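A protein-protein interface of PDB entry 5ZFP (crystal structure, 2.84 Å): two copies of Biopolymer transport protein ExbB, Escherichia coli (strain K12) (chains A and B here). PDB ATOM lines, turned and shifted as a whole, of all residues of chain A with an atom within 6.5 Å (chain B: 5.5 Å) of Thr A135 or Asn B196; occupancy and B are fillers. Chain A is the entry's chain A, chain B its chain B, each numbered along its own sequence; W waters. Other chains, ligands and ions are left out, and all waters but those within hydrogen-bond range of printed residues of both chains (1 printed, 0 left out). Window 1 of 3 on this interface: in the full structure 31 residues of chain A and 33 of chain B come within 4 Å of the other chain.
The guanidinium group (NH2) of Arg B200 lies close to the backbone NH (N) of Gly A131, at 3.3 Å.
The backbone carbonyl oxygen of Gly A131 lies within hydrogen-bond range of the side-chain hydroxyl of Thr A135 (3.0 Å). The backbone carbonyl oxygen (O) of Val B192 sits close to the side-chain amide oxygen (OD1) of Asn B196 (3.2 Å).
Thr A135 touches Asn B196 (OG1 to CB, 3.6 Å). Ile A139 touches Val B192. Ile A139 touches Val B193.
Thr A135 touches just one residue of chain B: Asn B196. Asn B196 touches one residue of chain A. Printed residues of chain A within 4 Å of Arg B200: Gly A131. Printed residues of chain A within 4 Å of Val B192: Ile A139. Tyr B195 touches none of the printed residues of chain A. The nearest residue of chain B that does not touch Thr A135 is Val B193 (4.1 Å). The nearest residue of chain A that does not touch Asn B196 is Ala A138 (4.6 Å).
Printed residues of chain B that touch a printed residue of chain A: Val B192, Val B193, Asn B196 and Arg B200. Of the 12 printed residues of chain A, 3 touch a printed residue of chain B. Printed residues of chain A that touch a printed residue of chain B: Gly A131, Thr A135 and Ile A139. Hydrophobic or aromatic side chains of chain A that line the printed part of chain B: Ile A139. Among the printed residues, no Asp or Glu carboxylate lies within 4 Å of a Lys or Arg side-chain nitrogen of the other chain.
No position is printed for both chains. Of the 4 pairs that touch across the chains among the printed residues, none has its exchanged pair printed and touching as well.
Water W1 bridges the guanidinium group of Arg B200 (3.3 Å) and the backbone NH of Gly A131 (3.4 Å).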
ATOM      1  N   ASN A 130     -20.101  -2.630  -2.233  1.00  0.00           N
ATOM      2  CA  ASN A 130     -20.428  -1.470  -1.410  1.00  0.00           C
ATOM      3  C   ASN A 130     -19.481  -1.294  -0.221  1.00  0.00           C
ATOM      4  O   ASN A 130     -19.311  -0.173   0.254  1.00  0.00           O
ATOM      5  CB  ASN A 130     -21.886  -1.510  -0.965  1.00  0.00           C
ATOM      6  CG  ASN A 130     -22.825  -0.922  -1.977  1.00  0.00           C
ATOM      7  OD1 ASN A 130     -23.158   0.259  -1.924  1.00  0.00           O
ATOM      8  ND2 ASN A 130     -23.255  -1.724  -2.929  1.00  0.00           N
ATOM      9  N   GLY A 131     -18.852  -2.387   0.216  1.00  0.00           N
ATOM     10  CA  GLY A 131     -17.873  -2.378   1.297  1.00  0.00           C
ATOM     11  C   GLY A 131     -16.650  -1.566   0.931  1.00  0.00           C
ATOM     12  O   GLY A 131     -16.110  -0.841   1.772  1.00  0.00           O
ATOM     13  N   TYR A 132     -16.239  -1.664  -0.348  1.00  0.00           N
ATOM     14  CA  TYR A 132     -15.126  -0.919  -0.917  1.00  0.00           C
ATOM     15  C   TYR A 132     -15.480   0.555  -1.004  1.00  0.00           C
ATOM     16  O   TYR A 132     -14.635   1.380  -0.669  1.00  0.00           O
ATOM     17  CB  TYR A 132     -14.772  -1.450  -2.308  1.00  0.00           C
ATOM     18  CG  TYR A 132     -13.918  -2.695  -2.292  1.00  0.00           C
ATOM     19  CD1 TYR A 132     -14.493  -3.958  -2.213  1.00  0.00           C
ATOM     20  CD2 TYR A 132     -12.534  -2.614  -2.403  1.00  0.00           C
ATOM     21  CE1 TYR A 132     -13.708  -5.113  -2.214  1.00  0.00           C
ATOM     22  CE2 TYR A 132     -11.737  -3.758  -2.399  1.00  0.00           C
ATOM     23  CZ  TYR A 132     -12.327  -5.007  -2.302  1.00  0.00           C
ATOM     24  OH  TYR A 132     -11.537  -6.135  -2.292  1.00  0.00           O
ATOM     25  N   LEU A 133     -16.732   0.895  -1.413  1.00  0.00           N
ATOM     26  CA  LEU A 133     -17.198   2.283  -1.529  1.00  0.00           C
ATOM     27  C   LEU A 133     -17.239   2.973  -0.157  1.00  0.00           C
ATOM     28  O   LEU A 133     -16.869   4.139  -0.042  1.00  0.00           O
ATOM     29  CB  LEU A 133     -18.550   2.375  -2.258  1.00  0.00           C
ATOM     30  CG  LEU A 133     -18.578   1.941  -3.729  1.00  0.00           C
ATOM     31  CD1 LEU A 133     -19.966   1.554  -4.159  1.00  0.00           C
ATOM     32  CD2 LEU A 133     -18.058   3.012  -4.635  1.00  0.00           C
ATOM     33  N   ALA A 134     -17.623   2.232   0.892  1.00  0.00           N
ATOM     34  CA  ALA A 134     -17.676   2.726   2.267  1.00  0.00           C
ATOM     35  C   ALA A 134     -16.247   3.005   2.816  1.00  0.00           C
ATOM     36  O   ALA A 134     -16.010   4.080   3.371  1.00  0.00           O
ATOM     37  CB  ALA A 134     -18.400   1.725   3.140  1.00  0.00           C
ATOM     38  N   THR A 135     -15.291   2.067   2.624  1.00  0.00           N
ATOM     39  CA  THR A 135     -13.897   2.246   3.067  1.00  0.00           C
ATOM     40  C   THR A 135     -13.209   3.403   2.313  1.00  0.00           C
ATOM     41  O   THR A 135     -12.533   4.201   2.955  1.00  0.00           O
ATOM     42  CB  THR A 135     -13.114   0.941   3.022  1.00  0.00           C
ATOM     43  OG1 THR A 135     -13.871  -0.081   3.674  1.00  0.00           O
ATOM     44  CG2 THR A 135     -11.754   1.055   3.685  1.00  0.00           C
ATOM     45  N   ILE A 136     -13.422   3.528   0.980  1.00  0.00           N
ATOM     46  CA  ILE A 136     -12.863   4.641   0.178  1.00  0.00           C
ATOM     47  C   ILE A 136     -13.413   6.008   0.657  1.00  0.00           C
ATOM     48  O   ILE A 136     -12.648   6.963   0.791  1.00  0.00           O
ATOM     49  CB  ILE A 136     -13.030   4.413  -1.346  1.00  0.00           C
ATOM     50  CG1 ILE A 136     -12.203   3.188  -1.786  1.00  0.00           C
ATOM     51  CG2 ILE A 136     -12.615   5.660  -2.143  1.00  0.00           C
ATOM     52  CD1 ILE A 136     -12.662   2.553  -3.017  1.00  0.00           C
ATOM     53  N   GLY A 137     -14.706   6.050   0.975  1.00  0.00           N
ATOM     54  CA  GLY A 137     -15.354   7.251   1.486  1.00  0.00           C
ATOM     55  C   GLY A 137     -14.823   7.648   2.852  1.00  0.00           C
ATOM     56  O   GLY A 137     -14.606   8.833   3.108  1.00  0.00           O
ATOM     57  N   ALA A 138     -14.566   6.643   3.720  1.00  0.00           N
ATOM     58  CA  ALA A 138     -14.081   6.810   5.094  1.00  0.00           C
ATOM     59  C   ALA A 138     -12.580   7.112   5.232  1.00  0.00           C
ATOM     60  O   ALA A 138     -12.232   7.918   6.094  1.00  0.00           O
ATOM     61  CB  ALA A 138     -14.451   5.599   5.927  1.00  0.00           C
ATOM     62  N   ILE A 139     -11.696   6.493   4.415  1.00  0.00           N
ATOM     63  CA  ILE A 139     -10.250   6.721   4.544  1.00  0.00           C
ATOM     64  C   ILE A 139      -9.717   7.862   3.659  1.00  0.00           C
ATOM     65  O   ILE A 139      -8.742   8.496   4.063  1.00  0.00           O
ATOM     66  CB  ILE A 139      -9.374   5.444   4.405  1.00  0.00           C
ATOM     67  CG1 ILE A 139      -9.395   4.836   3.000  1.00  0.00           C
ATOM     68  CG2 ILE A 139      -9.740   4.406   5.457  1.00  0.00           C
ATOM     69  CD1 ILE A 139      -8.013   4.288   2.535  1.00  0.00           C
ATOM     70  N   SER A 140     -10.348   8.149   2.496  1.00  0.00           N
ATOM     71  CA  SER A 140      -9.916   9.248   1.607  1.00  0.00           C
ATOM     72  C   SER A 140      -9.748  10.593   2.301  1.00  0.00           C
ATOM     73  O   SER A 140      -8.730  11.225   2.037  1.00  0.00           O
ATOM     74  CB  SER A 140     -10.820   9.397   0.395  1.00  0.00           C
ATOM     75  OG  SER A 140     -10.652   8.291  -0.474  1.00  0.00           O
ATOM     76  N   PRO A 141     -10.637  11.040   3.227  1.00  0.00           N
ATOM     77  CA  PRO A 141     -10.393  12.314   3.912  1.00  0.00           C
ATOM     78  C   PRO A 141      -9.163  12.292   4.803  1.00  0.00           C
ATOM     79  O   PRO A 141      -8.529  13.329   4.912  1.00  0.00           O
ATOM     80  CB  PRO A 141     -11.659  12.517   4.751  1.00  0.00           C
ATOM     81  CG  PRO A 141     -12.698  11.690   4.058  1.00  0.00           C
ATOM     82  CD  PRO A 141     -11.924  10.476   3.673  1.00  0.00           C
ATOM     83  N   ALA B 191      -5.683   0.709  10.801  1.00  0.00           N
ATOM     84  CA  ALA B 191      -6.684   0.252  11.782  1.00  0.00           C
ATOM     85  C   ALA B 191      -8.141   0.443  11.282  1.00  0.00           C
ATOM     86  O   ALA B 191      -8.982  -0.433  11.539  1.00  0.00           O
ATOM     87  CB  ALA B 191      -6.488   0.949  13.124  1.00  0.00           C
ATOM     88  N   VAL B 192      -8.424   1.578  10.554  1.00  0.00           N
ATOM     89  CA  VAL B 192      -9.737   1.917   9.969  1.00  0.00           C
ATOM     90  C   VAL B 192     -10.097   0.923   8.850  1.00  0.00           C
ATOM     91  O   VAL B 192     -11.203   0.375   8.842  1.00  0.00           O
ATOM     92  CB  VAL B 192      -9.810   3.395   9.503  1.00  0.00           C
ATOM     93  CG1 VAL B 192     -11.053   3.648   8.665  1.00  0.00           C
ATOM     94  CG2 VAL B 192      -9.774   4.353  10.694  1.00  0.00           C
ATOM     95  N   VAL B 193      -9.147   0.663   7.940  1.00  0.00           N
ATOM     96  CA  VAL B 193      -9.304  -0.274   6.815  1.00  0.00           C
ATOM     97  C   VAL B 193      -9.615  -1.705   7.329  1.00  0.00           C
ATOM     98  O   VAL B 193     -10.660  -2.282   6.993  1.00  0.00           O
ATOM     99  CB  VAL B 193      -8.055  -0.212   5.871  1.00  0.00           C
ATOM    100  CG1 VAL B 193      -8.114  -1.293   4.797  1.00  0.00           C
ATOM    101  CG2 VAL B 193      -7.906   1.168   5.232  1.00  0.00           C
ATOM    102  N   ILE B 194      -8.716  -2.233   8.182  1.00  0.00           N
ATOM    103  CA  ILE B 194      -8.796  -3.560   8.809  1.00  0.00           C
ATOM    104  C   ILE B 194     -10.089  -3.698   9.624  1.00  0.00           C
ATOM    105  O   ILE B 194     -10.749  -4.729   9.506  1.00  0.00           O
ATOM    106  CB  ILE B 194      -7.492  -3.863   9.624  1.00  0.00           C
ATOM    107  CG1 ILE B 194      -6.273  -3.971   8.698  1.00  0.00           C
ATOM    108  CG2 ILE B 194      -7.613  -5.124  10.454  1.00  0.00           C
ATOM    109  CD1 ILE B 194      -4.889  -3.723   9.393  1.00  0.00           C
ATOM    110  N   TYR B 195     -10.486  -2.647  10.404  1.00  0.00           N
ATOM    111  CA  TYR B 195     -11.742  -2.673  11.173  1.00  0.00           C
ATOM    112  C   TYR B 195     -12.949  -2.900  10.250  1.00  0.00           C
ATOM    113  O   TYR B 195     -13.805  -3.715  10.584  1.00  0.00           O
ATOM    114  CB  TYR B 195     -11.956  -1.399  12.020  1.00  0.00           C
ATOM    115  CG  TYR B 195     -13.346  -1.319  12.611  1.00  0.00           C
ATOM    116  CD1 TYR B 195     -13.674  -2.020  13.771  1.00  0.00           C
ATOM    117  CD2 TYR B 195     -14.361  -0.616  11.964  1.00  0.00           C
ATOM    118  CE1 TYR B 195     -14.975  -2.013  14.278  1.00  0.00           C
ATOM    119  CE2 TYR B 195     -15.665  -0.607  12.458  1.00  0.00           C
ATOM    120  CZ  TYR B 195     -15.967  -1.301  13.617  1.00  0.00           C
ATOM    121  OH  TYR B 195     -17.256  -1.264  14.100  1.00  0.00           O
ATOM    122  N   ASN B 196     -13.017  -2.170   9.108  1.00  0.00           N
ATOM    123  CA  ASN B 196     -14.115  -2.270   8.151  1.00  0.00           C
ATOM    124  C   ASN B 196     -14.186  -3.615   7.420  1.00  0.00           C
ATOM    125  O   ASN B 196     -15.293  -4.132   7.199  1.00  0.00           O
ATOM    126  CB  ASN B 196     -14.102  -1.099   7.168  1.00  0.00           C
ATOM    127  CG  ASN B 196     -14.484   0.232   7.785  1.00  0.00           C
ATOM    128  OD1 ASN B 196     -13.911   1.274   7.449  1.00  0.00           O
ATOM    129  ND2 ASN B 196     -15.463   0.245   8.693  1.00  0.00           N
ATOM    130  N   VAL B 197     -13.019  -4.197   7.072  1.00  0.00           N
ATOM    131  CA  VAL B 197     -13.001  -5.490   6.384  1.00  0.00           C
ATOM    132  C   VAL B 197     -13.560  -6.570   7.327  1.00  0.00           C
ATOM    133  O   VAL B 197     -14.488  -7.294   6.941  1.00  0.00           O
ATOM    134  CB  VAL B 197     -11.637  -5.869   5.694  1.00  0.00           C
ATOM    135  CG1 VAL B 197     -11.132  -4.763   4.760  1.00  0.00           C
ATOM    136  CG2 VAL B 197     -10.557  -6.232   6.679  1.00  0.00           C
ATOM    137  N   PHE B 198     -13.074  -6.584   8.590  1.00  0.00           N
ATOM    138  CA  PHE B 198     -13.507  -7.532   9.616  1.00  0.00           C
ATOM    139  C   PHE B 198     -14.971  -7.372   9.995  1.00  0.00           C
ATOM    140  O   PHE B 198     -15.662  -8.387  10.120  1.00  0.00           O
ATOM    141  CB  PHE B 198     -12.604  -7.478  10.859  1.00  0.00           C
ATOM    142  CG  PHE B 198     -11.199  -8.015  10.702  1.00  0.00           C
ATOM    143  CD1 PHE B 198     -10.871  -8.866   9.648  1.00  0.00           C
ATOM    144  CD2 PHE B 198     -10.212  -7.707  11.633  1.00  0.00           C
ATOM    145  CE1 PHE B 198      -9.572  -9.360   9.502  1.00  0.00           C
ATOM    146  CE2 PHE B 198      -8.913  -8.200  11.489  1.00  0.00           C
ATOM    147  CZ  PHE B 198      -8.597  -9.013  10.417  1.00  0.00           C
ATOM    148  N   ALA B 199     -15.463  -6.112  10.140  1.00  0.00           N
ATOM    149  CA  ALA B 199     -16.864  -5.821  10.481  1.00  0.00           C
ATOM    150  C   ALA B 199     -17.809  -6.403   9.446  1.00  0.00           C
ATOM    151  O   ALA B 199     -18.870  -6.900   9.818  1.00  0.00           O
ATOM    152  CB  ALA B 199     -17.090  -4.322  10.594  1.00  0.00           C
ATOM    153  N   ARG B 200     -17.408  -6.348   8.150  1.00  0.00           N
ATOM    154  CA  ARG B 200     -18.161  -6.870   7.010  1.00  0.00           C
ATOM    155  C   ARG B 200     -18.173  -8.392   7.040  1.00  0.00           C
ATOM    156  O   ARG B 200     -19.236  -8.996   6.832  1.00  0.00           O
ATOM    157  CB  ARG B 200     -17.578  -6.358   5.680  1.00  0.00           C
ATOM    158  CG  ARG B 200     -18.089  -4.976   5.292  1.00  0.00           C
ATOM    159  CD  ARG B 200     -17.929  -4.671   3.810  1.00  0.00           C
ATOM    160  NE  ARG B 200     -18.677  -5.586   2.919  1.00  0.00           N
ATOM    161  CZ  ARG B 200     -19.856  -5.331   2.347  1.00  0.00           C
ATOM    162  NH1 ARG B 200     -20.435  -6.242   1.576  1.00  0.00           N
ATOM    163  NH2 ARG B 200     -20.465  -4.169   2.548  1.00  0.00           N
ATOM    164  N   GLN B 201     -16.997  -9.003   7.309  1.00  0.00           N
ATOM    165  CA  GLN B 201     -16.802 -10.449   7.383  1.00  0.00           C
ATOM    166  C   GLN B 201     -17.626 -11.074   8.515  1.00  0.00           C
ATOM    167  O   GLN B 201     -18.274 -12.101   8.295  1.00  0.00           O
ATOM    168  CB  GLN B 201     -15.304 -10.787   7.538  1.00  0.00           C
ATOM    169  CG  GLN B 201     -14.442 -10.504   6.315  1.00  0.00           C
ATOM    170  CD  GLN B 201     -13.103 -11.184   6.454  1.00  0.00           C
ATOM    171  OE1 GLN B 201     -12.179 -10.685   7.110  1.00  0.00           O
ATOM    172  NE2 GLN B 201     -12.993 -12.391   5.907  1.00  0.00           N
HETATM  173  O   HOH W   1     -17.900  -5.600  -0.375  1.00  0.00           O
